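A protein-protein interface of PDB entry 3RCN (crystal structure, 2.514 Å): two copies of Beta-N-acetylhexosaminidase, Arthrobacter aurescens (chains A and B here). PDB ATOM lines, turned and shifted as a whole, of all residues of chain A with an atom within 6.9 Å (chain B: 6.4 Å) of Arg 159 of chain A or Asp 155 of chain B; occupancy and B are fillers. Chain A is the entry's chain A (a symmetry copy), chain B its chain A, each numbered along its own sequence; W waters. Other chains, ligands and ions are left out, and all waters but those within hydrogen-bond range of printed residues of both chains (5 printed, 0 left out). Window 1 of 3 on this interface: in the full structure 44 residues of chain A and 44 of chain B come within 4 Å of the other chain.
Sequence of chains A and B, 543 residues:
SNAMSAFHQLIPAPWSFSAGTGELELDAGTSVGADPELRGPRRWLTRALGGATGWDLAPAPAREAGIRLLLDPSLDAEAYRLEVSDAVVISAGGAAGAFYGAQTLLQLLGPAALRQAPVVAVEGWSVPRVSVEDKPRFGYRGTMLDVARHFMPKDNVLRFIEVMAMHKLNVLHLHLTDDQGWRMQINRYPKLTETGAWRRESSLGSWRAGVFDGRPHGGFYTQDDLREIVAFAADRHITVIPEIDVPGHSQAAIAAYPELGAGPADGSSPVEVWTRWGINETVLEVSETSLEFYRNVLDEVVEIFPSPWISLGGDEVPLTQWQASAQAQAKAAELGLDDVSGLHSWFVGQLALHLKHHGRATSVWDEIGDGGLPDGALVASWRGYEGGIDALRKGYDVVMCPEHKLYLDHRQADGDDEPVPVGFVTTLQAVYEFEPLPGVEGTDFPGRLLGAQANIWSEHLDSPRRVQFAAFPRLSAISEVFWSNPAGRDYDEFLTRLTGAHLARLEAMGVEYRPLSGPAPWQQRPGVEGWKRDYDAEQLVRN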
ATOM      1  N   LEU A 114      18.767  -5.143  17.330  1.00  0.00           N
ATOM      2  CA  LEU A 114      19.440  -6.285  17.969  1.00  0.00           C
ATOM      3  C   LEU A 114      19.089  -7.661  17.402  1.00  0.00           C
ATOM      4  O   LEU A 114      19.624  -8.679  17.851  1.00  0.00           O
ATOM      5  CB  LEU A 114      19.130  -6.297  19.465  1.00  0.00           C
ATOM      6  CG  LEU A 114      19.484  -4.983  20.148  1.00  0.00           C
ATOM      7  CD1 LEU A 114      18.993  -4.965  21.579  1.00  0.00           C
ATOM      8  CD2 LEU A 114      20.979  -4.791  20.077  1.00  0.00           C
ATOM      9  N   ARG A 115      18.169  -7.701  16.441  1.00  0.00           N
ATOM     10  CA  ARG A 115      17.821  -8.954  15.789  1.00  0.00           C
ATOM     11  C   ARG A 115      18.917  -9.375  14.810  1.00  0.00           C
ATOM     12  O   ARG A 115      19.701  -8.551  14.353  1.00  0.00           O
ATOM     13  CB  ARG A 115      16.476  -8.825  15.072  1.00  0.00           C
ATOM     14  CG  ARG A 115      15.334  -8.395  15.976  1.00  0.00           C
ATOM     15  CD  ARG A 115      14.723  -9.571  16.715  1.00  0.00           C
ATOM     16  NE  ARG A 115      13.642  -9.154  17.607  1.00  0.00           N
ATOM     17  CZ  ARG A 115      12.876  -9.998  18.295  1.00  0.00           C
ATOM     18  NH1 ARG A 115      13.063 -11.306  18.184  1.00  0.00           N
ATOM     19  NH2 ARG A 115      11.912  -9.535  19.082  1.00  0.00           N
ATOM     20  N   GLN A 116      18.961 -10.659  14.482  1.00  0.00           N
ATOM     21  CA  GLN A 116      19.938 -11.176  13.526  1.00  0.00           C
ATOM     22  C   GLN A 116      19.421 -11.153  12.082  1.00  0.00           C
ATOM     23  O   GLN A 116      20.165 -11.444  11.155  1.00  0.00           O
ATOM     24  CB  GLN A 116      20.393 -12.588  13.931  1.00  0.00           C
ATOM     25  CG  GLN A 116      21.048 -12.668  15.332  1.00  0.00           C
ATOM     26  CD  GLN A 116      21.466 -14.091  15.725  1.00  0.00           C
ATOM     27  OE1 GLN A 116      22.132 -14.800  14.959  1.00  0.00           O
ATOM     28  NE2 GLN A 116      21.064 -14.516  16.922  1.00  0.00           N
ATOM     29  N   LYS A 154      28.878 -24.464  22.841  1.00  0.00           N
ATOM     30  CA  LYS A 154      29.569 -23.320  22.254  1.00  0.00           C
ATOM     31  C   LYS A 154      28.629 -22.247  21.665  1.00  0.00           C
ATOM     32  O   LYS A 154      28.856 -21.046  21.857  1.00  0.00           O
ATOM     33  CB  LYS A 154      30.553 -23.827  21.202  1.00  0.00           C
ATOM     34  CG  LYS A 154      31.392 -22.757  20.534  1.00  0.00           C
ATOM     35  CD  LYS A 154      32.546 -23.392  19.770  1.00  0.00           C
ATOM     36  CE  LYS A 154      32.080 -24.139  18.509  1.00  0.00           C
ATOM     37  NZ  LYS A 154      31.643 -23.202  17.436  1.00  0.00           N
ATOM     38  N   ASP A 155      27.587 -22.675  20.948  1.00  0.00           N
ATOM     39  CA  ASP A 155      26.599 -21.749  20.381  1.00  0.00           C
ATOM     40  C   ASP A 155      26.008 -20.808  21.446  1.00  0.00           C
ATOM     41  O   ASP A 155      25.819 -19.613  21.216  1.00  0.00           O
ATOM     42  CB  ASP A 155      25.462 -22.518  19.677  1.00  0.00           C
ATOM     43  CG  ASP A 155      25.884 -23.120  18.320  1.00  0.00           C
ATOM     44  OD1 ASP A 155      25.183 -24.049  17.824  1.00  0.00           O
ATOM     45  OD2 ASP A 155      26.908 -22.662  17.752  1.00  0.00           O
ATOM     46  N   ASN A 156      25.728 -21.364  22.617  1.00  0.00           N
ATOM     47  CA  ASN A 156      25.150 -20.608  23.717  1.00  0.00           C
ATOM     48  C   ASN A 156      26.158 -19.692  24.418  1.00  0.00           C
ATOM     49  O   ASN A 156      25.815 -18.571  24.815  1.00  0.00           O
ATOM     50  CB  ASN A 156      24.472 -21.562  24.694  1.00  0.00           C
ATOM     51  CG  ASN A 156      23.389 -22.389  24.021  1.00  0.00           C
ATOM     52  OD1 ASN A 156      23.597 -23.551  23.657  1.00  0.00           O
ATOM     53  ND2 ASN A 156      22.240 -21.774  23.808  1.00  0.00           N
ATOM     54  N   VAL A 157      27.400 -20.161  24.551  1.00  0.00           N
ATOM     55  CA  VAL A 157      28.481 -19.324  25.080  1.00  0.00           C
ATOM     56  C   VAL A 157      28.677 -18.047  24.242  1.00  0.00           C
ATOM     57  O   VAL A 157      28.811 -16.959  24.797  1.00  0.00           O
ATOM     58  CB  VAL A 157      29.842 -20.091  25.174  1.00  0.00           C
ATOM     59  CG1 VAL A 157      30.967 -19.155  25.620  1.00  0.00           C
ATOM     60  CG2 VAL A 157      29.749 -21.298  26.111  1.00  0.00           C
ATOM     61  N   LEU A 158      28.687 -18.166  22.915  1.00  0.00           N
ATOM     62  CA  LEU A 158      28.945 -16.992  22.090  1.00  0.00           C
ATOM     63  C   LEU A 158      27.774 -16.038  22.217  1.00  0.00           C
ATOM     64  O   LEU A 158      27.945 -14.812  22.148  1.00  0.00           O
ATOM     65  CB  LEU A 158      29.155 -17.371  20.633  1.00  0.00           C
ATOM     66  CG  LEU A 158      30.210 -18.446  20.404  1.00  0.00           C
ATOM     67  CD1 LEU A 158      30.189 -18.964  18.966  1.00  0.00           C
ATOM     68  CD2 LEU A 158      31.592 -17.903  20.790  1.00  0.00           C
ATOM     69  N   ARG A 159      26.581 -16.601  22.400  1.00  0.00           N
ATOM     70  CA  ARG A 159      25.383 -15.768  22.555  1.00  0.00           C
ATOM     71  C   ARG A 159      25.363 -15.045  23.891  1.00  0.00           C
ATOM     72  O   ARG A 159      25.005 -13.868  23.973  1.00  0.00           O
ATOM     73  CB  ARG A 159      24.110 -16.596  22.381  1.00  0.00           C
ATOM     74  CG  ARG A 159      23.657 -16.686  20.940  1.00  0.00           C
ATOM     75  CD  ARG A 159      22.672 -15.585  20.633  1.00  0.00           C
ATOM     76  NE  ARG A 159      23.265 -14.499  19.884  1.00  0.00           N
ATOM     77  CZ  ARG A 159      22.676 -13.325  19.703  1.00  0.00           C
ATOM     78  NH1 ARG A 159      21.488 -13.099  20.233  1.00  0.00           N
ATOM     79  NH2 ARG A 159      23.282 -12.365  19.013  1.00  0.00           N
ATOM     80  N   PHE A 160      25.744 -15.758  24.943  1.00  0.00           N
ATOM     81  CA  PHE A 160      25.935 -15.143  26.248  1.00  0.00           C
ATOM     82  C   PHE A 160      26.967 -14.007  26.178  1.00  0.00           C
ATOM     83  O   PHE A 160      26.781 -12.949  26.784  1.00  0.00           O
ATOM     84  CB  PHE A 160      26.372 -16.207  27.253  1.00  0.00           C
ATOM     85  CG  PHE A 160      26.584 -15.682  28.650  1.00  0.00           C
ATOM     86  CD1 PHE A 160      25.513 -15.557  29.527  1.00  0.00           C
ATOM     87  CD2 PHE A 160      27.855 -15.321  29.088  1.00  0.00           C
ATOM     88  CE1 PHE A 160      25.700 -15.071  30.804  1.00  0.00           C
ATOM     89  CE2 PHE A 160      28.050 -14.836  30.369  1.00  0.00           C
ATOM     90  CZ  PHE A 160      26.971 -14.715  31.228  1.00  0.00           C
ATOM     91  N   ILE A 161      28.044 -14.220  25.426  1.00  0.00           N
ATOM     92  CA  ILE A 161      29.091 -13.206  25.280  1.00  0.00           C
ATOM     93  C   ILE A 161      28.568 -11.974  24.538  1.00  0.00           C
ATOM     94  O   ILE A 161      28.901 -10.841  24.882  1.00  0.00           O
ATOM     95  CB  ILE A 161      30.325 -13.762  24.542  1.00  0.00           C
ATOM     96  CG1 ILE A 161      31.132 -14.664  25.474  1.00  0.00           C
ATOM     97  CG2 ILE A 161      31.189 -12.627  24.019  1.00  0.00           C
ATOM     98  CD1 ILE A 161      32.172 -15.522  24.767  1.00  0.00           C
ATOM     99  N   GLU A 162      27.731 -12.204  23.532  1.00  0.00           N
ATOM    100  CA  GLU A 162      27.141 -11.120  22.754  1.00  0.00           C
ATOM    101  C   GLU A 162      26.240 -10.243  23.626  1.00  0.00           C
ATOM    102  O   GLU A 162      26.255  -9.005  23.531  1.00  0.00           O
ATOM    103  CB  GLU A 162      26.349 -11.704  21.581  1.00  0.00           C
ATOM    104  CG  GLU A 162      25.802 -10.662  20.625  1.00  0.00           C
ATOM    105  CD  GLU A 162      26.835 -10.163  19.621  1.00  0.00           C
ATOM    106  OE1 GLU A 162      26.888 -10.751  18.515  1.00  0.00           O
ATOM    107  OE2 GLU A 162      27.574  -9.184  19.922  1.00  0.00           O
ATOM    108  N   VAL A 163      25.451 -10.892  24.479  1.00  0.00           N
ATOM    109  CA  VAL A 163      24.605 -10.175  25.429  1.00  0.00           C
ATOM    110  C   VAL A 163      25.441  -9.403  26.457  1.00  0.00           C
ATOM    111  O   VAL A 163      25.052  -8.313  26.882  1.00  0.00           O
ATOM    112  CB  VAL A 163      23.624 -11.120  26.142  1.00  0.00           C
ATOM    113  CG1 VAL A 163      22.835 -10.373  27.189  1.00  0.00           C
ATOM    114  CG2 VAL A 163      22.677 -11.773  25.125  1.00  0.00           C
ATOM    115  N   MET A 164      26.588  -9.959  26.848  1.00  0.00           N
ATOM    116  CA  MET A 164      27.504  -9.255  27.758  1.00  0.00           C
ATOM    117  C   MET A 164      28.025  -7.951  27.161  1.00  0.00           C
ATOM    118  O   MET A 164      28.052  -6.919  27.826  1.00  0.00           O
ATOM    119  CB  MET A 164      28.717 -10.115  28.115  1.00  0.00           C
ATOM    120  CG  MET A 164      28.479 -11.232  29.100  1.00  0.00           C
ATOM    121  SD  MET A 164      30.166 -12.190  29.407  1.00  0.00           S
ATOM    122  CE  MET A 164      31.307 -10.811  30.161  1.00  0.00           C
ATOM    123  N   PHE A 232      36.093 -14.372  19.542  1.00  0.00           N
ATOM    124  CA  PHE A 232      34.746 -13.810  19.569  1.00  0.00           C
ATOM    125  C   PHE A 232      34.673 -12.740  20.660  1.00  0.00           C
ATOM    126  O   PHE A 232      34.216 -11.621  20.415  1.00  0.00           O
ATOM    127  CB  PHE A 232      33.708 -14.931  19.793  1.00  0.00           C
ATOM    128  CG  PHE A 232      32.271 -14.518  19.567  1.00  0.00           C
ATOM    129  CD1 PHE A 232      31.500 -14.026  20.609  1.00  0.00           C
ATOM    130  CD2 PHE A 232      31.674 -14.671  18.328  1.00  0.00           C
ATOM    131  CE1 PHE A 232      30.163 -13.677  20.412  1.00  0.00           C
ATOM    132  CE2 PHE A 232      30.344 -14.304  18.120  1.00  0.00           C
ATOM    133  CZ  PHE A 232      29.594 -13.813  19.164  1.00  0.00           C
ATOM    134  N   GLN A 468      20.038 -18.135  31.751  1.00  0.00           N
ATOM    135  CA  GLN A 468      19.488 -16.825  31.387  1.00  0.00           C
ATOM    136  C   GLN A 468      18.522 -16.313  32.452  1.00  0.00           C
ATOM    137  O   GLN A 468      18.456 -15.116  32.754  1.00  0.00           O
ATOM    138  CB  GLN A 468      18.784 -16.898  30.030  1.00  0.00           C
ATOM    139  CG  GLN A 468      19.731 -17.171  28.882  1.00  0.00           C
ATOM    140  CD  GLN A 468      19.019 -17.212  27.557  1.00  0.00           C
ATOM    141  OE1 GLN A 468      17.831 -17.535  27.487  1.00  0.00           O
ATOM    142  NE2 GLN A 468      19.734 -16.868  26.491  1.00  0.00           N
ATOM    143  N   ALA A 508      14.729  -9.353  22.282  1.00  0.00           N
ATOM    144  CA  ALA A 508      15.233  -9.341  20.920  1.00  0.00           C
ATOM    145  C   ALA A 508      16.525 -10.163  20.772  1.00  0.00           C
ATOM    146  O   ALA A 508      16.820 -10.678  19.694  1.00  0.00           O
ATOM    147  CB  ALA A 508      15.433  -7.896  20.440  1.00  0.00           C
ATOM    148  N   MET A 509      17.284 -10.284  21.857  1.00  0.00           N
ATOM    149  CA  MET A 509      18.557 -11.009  21.832  1.00  0.00           C
ATOM    150  C   MET A 509      18.405 -12.477  22.226  1.00  0.00           C
ATOM    151  O   MET A 509      19.395 -13.195  22.379  1.00  0.00           O
ATOM    152  CB  MET A 509      19.597 -10.328  22.731  1.00  0.00           C
ATOM    153  CG  MET A 509      19.948  -8.909  22.308  1.00  0.00           C
ATOM    154  SD  MET A 509      21.594  -8.230  23.124  1.00  0.00           S
ATOM    155  CE  MET A 509      22.876  -9.122  21.950  1.00  0.00           C
ATOM    156  N   GLY A 510      17.166 -12.912  22.422  1.00  0.00           N
ATOM    157  CA  GLY A 510      16.893 -14.302  22.742  1.00  0.00           C
ATOM    158  C   GLY A 510      17.077 -14.666  24.205  1.00  0.00           C
ATOM    159  O   GLY A 510      17.260 -15.834  24.548  1.00  0.00           O
ATOM    160  N   VAL A 511      17.011 -13.682  25.087  1.00  0.00           N
ATOM    161  CA  VAL A 511      17.285 -13.950  26.489  1.00  0.00           C
ATOM    162  C   VAL A 511      15.989 -14.151  27.257  1.00  0.00           C
ATOM    163  O   VAL A 511      15.200 -13.223  27.359  1.00  0.00           O
ATOM    164  CB  VAL A 511      18.065 -12.763  27.129  1.00  0.00           C
ATOM    165  CG1 VAL A 511      18.303 -13.015  28.600  1.00  0.00           C
ATOM    166  CG2 VAL A 511      19.378 -12.534  26.401  1.00  0.00           C
ATOM    167  N   MET B 152      12.291 -25.223  21.276  1.00  0.00           N
ATOM    168  CA  MET B 152      13.680 -24.886  21.020  1.00  0.00           C
ATOM    169  C   MET B 152      13.886 -23.371  21.110  1.00  0.00           C
ATOM    170  O   MET B 152      13.247 -22.599  20.396  1.00  0.00           O
ATOM    171  CB  MET B 152      14.149 -25.420  19.670  1.00  0.00           C
ATOM    172  CG  MET B 152      15.612 -25.098  19.412  1.00  0.00           C
ATOM    173  SD  MET B 152      16.415 -25.912  17.831  1.00  0.00           S
ATOM    174  CE  MET B 152      16.530 -27.754  18.496  1.00  0.00           C
ATOM    175  N   PRO B 153      14.767 -22.937  22.015  1.00  0.00           N
ATOM    176  CA  PRO B 153      14.972 -21.495  22.120  1.00  0.00           C
ATOM    177  C   PRO B 153      15.413 -20.898  20.785  1.00  0.00           C
ATOM    178  O   PRO B 153      16.081 -21.563  19.987  1.00  0.00           O
ATOM    179  CB  PRO B 153      16.068 -21.382  23.172  1.00  0.00           C
ATOM    180  CG  PRO B 153      15.920 -22.655  24.000  1.00  0.00           C
ATOM    181  CD  PRO B 153      15.572 -23.692  22.990  1.00  0.00           C
ATOM    182  N   LYS B 154      15.004 -19.653  20.555  1.00  0.00           N
ATOM    183  CA  LYS B 154      15.259 -18.941  19.306  1.00  0.00           C
ATOM    184  C   LYS B 154      16.735 -18.963  18.856  1.00  0.00           C
ATOM    185  O   LYS B 154      17.021 -19.155  17.668  1.00  0.00           O
ATOM    186  CB  LYS B 154      14.746 -17.509  19.444  1.00  0.00           C
ATOM    187  CG  LYS B 154      14.892 -16.650  18.205  1.00  0.00           C
ATOM    188  CD  LYS B 154      14.059 -15.380  18.344  1.00  0.00           C
ATOM    189  CE  LYS B 154      14.645 -14.400  19.374  1.00  0.00           C
ATOM    190  NZ  LYS B 154      15.890 -13.750  18.880  1.00  0.00           N
ATOM    191  N   ASP B 155      17.663 -18.758  19.795  1.00  0.00           N
ATOM    192  CA  ASP B 155      19.099 -18.804  19.493  1.00  0.00           C
ATOM    193  C   ASP B 155      19.502 -20.114  18.792  1.00  0.00           C
ATOM    194  O   ASP B 155      20.295 -20.123  17.850  1.00  0.00           O
ATOM    195  CB  ASP B 155      19.939 -18.620  20.773  1.00  0.00           C
ATOM    196  CG  ASP B 155      19.951 -17.165  21.288  1.00  0.00           C
ATOM    197  OD1 ASP B 155      20.289 -16.948  22.487  1.00  0.00           O
ATOM    198  OD2 ASP B 155      19.630 -16.244  20.494  1.00  0.00           O
ATOM    199  N   ASN B 156      18.936 -21.219  19.261  1.00  0.00           N
ATOM    200  CA  ASN B 156      19.229 -22.533  18.713  1.00  0.00           C
ATOM    201  C   ASN B 156      18.556 -22.791  17.361  1.00  0.00           C
ATOM    202  O   ASN B 156      19.152 -23.416  16.475  1.00  0.00           O
ATOM    203  CB  ASN B 156      18.875 -23.606  19.739  1.00  0.00           C
ATOM    204  CG  ASN B 156      19.633 -23.418  21.042  1.00  0.00           C
ATOM    205  OD1 ASN B 156      19.106 -22.878  22.021  1.00  0.00           O
ATOM    206  ND2 ASN B 156      20.891 -23.819  21.043  1.00  0.00           N
ATOM    207  N   VAL B 157      17.331 -22.293  17.200  1.00  0.00           N
ATOM    208  CA  VAL B 157      16.643 -22.355  15.906  1.00  0.00           C
ATOM    209  C   VAL B 157      17.452 -21.660  14.796  1.00  0.00           C
ATOM    210  O   VAL B 157      17.595 -22.204  13.703  1.00  0.00           O
ATOM    211  CB  VAL B 157      15.206 -21.738  15.959  1.00  0.00           C
ATOM    212  CG1 VAL B 157      14.569 -21.718  14.568  1.00  0.00           C
ATOM    213  CG2 VAL B 157      14.306 -22.481  16.949  1.00  0.00           C
ATOM    214  N   LEU B 158      17.988 -20.470  15.064  1.00  0.00           N
ATOM    215  CA  LEU B 158      18.697 -19.747  14.015  1.00  0.00           C
ATOM    216  C   LEU B 158      19.974 -20.494  13.683  1.00  0.00           C
ATOM    217  O   LEU B 158      20.432 -20.484  12.531  1.00  0.00           O
ATOM    218  CB  LEU B 158      19.019 -18.323  14.440  1.00  0.00           C
ATOM    219  CG  LEU B 158      17.822 -17.527  14.945  1.00  0.00           C
ATOM    220  CD1 LEU B 158      18.250 -16.212  15.594  1.00  0.00           C
ATOM    221  CD2 LEU B 158      16.835 -17.296  13.793  1.00  0.00           C
ATOM    222  N   ARG B 159      20.550 -21.141  14.695  1.00  0.00           N
ATOM    223  CA  ARG B 159      21.779 -21.911  14.478  1.00  0.00           C
ATOM    224  C   ARG B 159      21.523 -23.177  13.680  1.00  0.00           C
ATOM    225  O   ARG B 159      22.297 -23.536  12.790  1.00  0.00           O
ATOM    226  CB  ARG B 159      22.457 -22.250  15.806  1.00  0.00           C
ATOM    227  CG  ARG B 159      23.413 -21.173  16.272  1.00  0.00           C
ATOM    228  CD  ARG B 159      24.810 -21.468  15.782  1.00  0.00           C
ATOM    229  NE  ARG B 159      25.187 -20.650  14.651  1.00  0.00           N
ATOM    230  CZ  ARG B 159      26.256 -20.882  13.900  1.00  0.00           C
ATOM    231  NH1 ARG B 159      27.032 -21.916  14.168  1.00  0.00           N
ATOM    232  NH2 ARG B 159      26.538 -20.097  12.867  1.00  0.00           N
ATOM    233  N   PHE B 160      20.432 -23.858  14.004  1.00  0.00           N
ATOM    234  CA  PHE B 160      19.978 -24.989  13.209  1.00  0.00           C
ATOM    235  C   PHE B 160      19.735 -24.576  11.749  1.00  0.00           C
ATOM    236  O   PHE B 160      20.087 -25.308  10.821  1.00  0.00           O
ATOM    237  CB  PHE B 160      18.705 -25.566  13.825  1.00  0.00           C
ATOM    238  CG  PHE B 160      18.153 -26.759  13.088  1.00  0.00           C
ATOM    239  CD1 PHE B 160      18.637 -28.036  13.349  1.00  0.00           C
ATOM    240  CD2 PHE B 160      17.144 -26.605  12.141  1.00  0.00           C
ATOM    241  CE1 PHE B 160      18.138 -29.131  12.674  1.00  0.00           C
ATOM    242  CE2 PHE B 160      16.638 -27.700  11.463  1.00  0.00           C
ATOM    243  CZ  PHE B 160      17.135 -28.964  11.732  1.00  0.00           C
HETATM  244  O   HOH W   1      21.893 -17.538  17.459  1.00  0.00           O
HETATM  245  O   HOH W   2      18.502 -14.012  18.571  1.00  0.00           O
HETATM  246  O   HOH W   3      21.179 -19.031  24.341  1.00  0.00           O
HETATM  247  O   HOH W   4      17.037 -18.105  22.434  1.00  0.00           O
HETATM  248  O   HOH W   5      22.716 -25.062  19.029  1.00  0.00           O
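Along chain A the printed residues that touch a printed residue of chain B span positions 115 to 510. Along chain B the printed residues that touch a printed residue of chain A span positions 154 to 159. Among the printed residues, 9 pairs touch across the chains. Among the printed residues, Asp or Glu carboxylates within 4 Å of a Lys or Arg side-chain nitrogen of the other chain: Asp 155 of chain A with Arg 159 of chain B and Arg 159 of chain A with Asp 155 of chain B.
Among the printed residues, pairs that only touch across the chains: Arg 115 of chain A with Lys 154 of chain B (3.7 Å), Gln 116 of chain A with Leu 158 of chain B (3.5 Å), Asn 156 of chain A with Asn 156 of chain B (3.7 Å), Met 509 of chain A with Asp 155 of chain B (3.6 Å), Gly 510 of chain A with Lys 154 of chain B (3.9 Å) and Gly 510 of chain A with Asp 155 of chain B (3.8 Å).
The backbone carbonyl oxygen (O) of Gly 510 of chain A is in hydrogen-bond range of the side-chain amide nitrogen (NE2) of Gln 468 of chain A. The guanidinium group (NH2) of Arg 159 of chain A is in salt-bridge range of the side-chain carboxylate (OE1) of Glu 162 of chain A, at 3.98 Å. The guanidinium group (NH1) of Arg 159 of chain A is in hydrogen-bond range of the backbone carbonyl oxygen (O) of Met 509 of chain A (3.0 Å).
Of chain B, only Asp 155 comes within 4 Å of Arg 159 of chain A. Of the printed residues of chain B, Asp 155 of chain A touches Arg 159 (3.1 Å). Printed residues of chain B within 4 Å of Gly 510 of chain A: Lys 154 and Asp 155. The nearest residue of chain B that does not touch Arg 159 of chain A is Lys 154 of chain B (5.8 Å).
Asp 155 of chain A touches Arg 159 of chain B, and with the chains exchanged Arg 159 of chain A touches Asp 155 of chain B. Asn 156 of chain A touches its own counterpart, Asn 156 of chain B. Positions printed for both chains: 154, 155, 156, 157, 158, 159 and 160. Of the 9 pairs that touch across the chains among the printed residues, 3 have their exchanged pair printed and touching as well.
Water W2 lies within hydrogen-bond range of the side-chain amino group of Lys 154 of chain B (2.6 Å), the side-chain amide nitrogen of Gln 116 of chain A (3.1 Å) and the side-chain carboxylate of Asp 155 of chain B (3.2 Å). Water W4 lies within hydrogen-bond range of the backbone NH (N) of Asp 155 of chain B (2.8 Å), the backbone carbonyl oxygen (O) of Gly 510 of chain A (3.1 Å) and the backbone NH (N) of Lys 154 of chain B (3.2 Å). Water W3 lies within hydrogen-bond range of the side-chain carboxylate of Asp 155 of chain B (2.9 Å), the side-chain amide nitrogen of Asn 156 of chain A (3.0 Å) and the side-chain amide nitrogen of Gln 468 of chain A (3.4 Å). Water W5 lies within hydrogen-bond range of the side-chain carboxylate of Asp 155 of chain A and the side-chain amide nitrogen of Asn 156 of chain B. Water W1 lies within hydrogen-bond range of O of Asp 155 of chain B (3.1 Å) and NE2 of Gln 116 of chain A (3.2 Å).
The side-chain amino group (NZ) of Lys 154 of chain B lies within hydrogen-bond range of the backbone carbonyl oxygen (O) of Ala 508 of chain A, 3.3 Å away. The side-chain carboxylate (OD2) of Asp 155 of chain B is in salt-bridge range of the guanidinium group (NH1) of Arg 159 of chain A, 3.7 Å away. The guanidinium group (NH1) of Arg 159 of chain B lies within salt-bridge range of the side-chain carboxylate (OD2) of Asp 155 of chain A.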
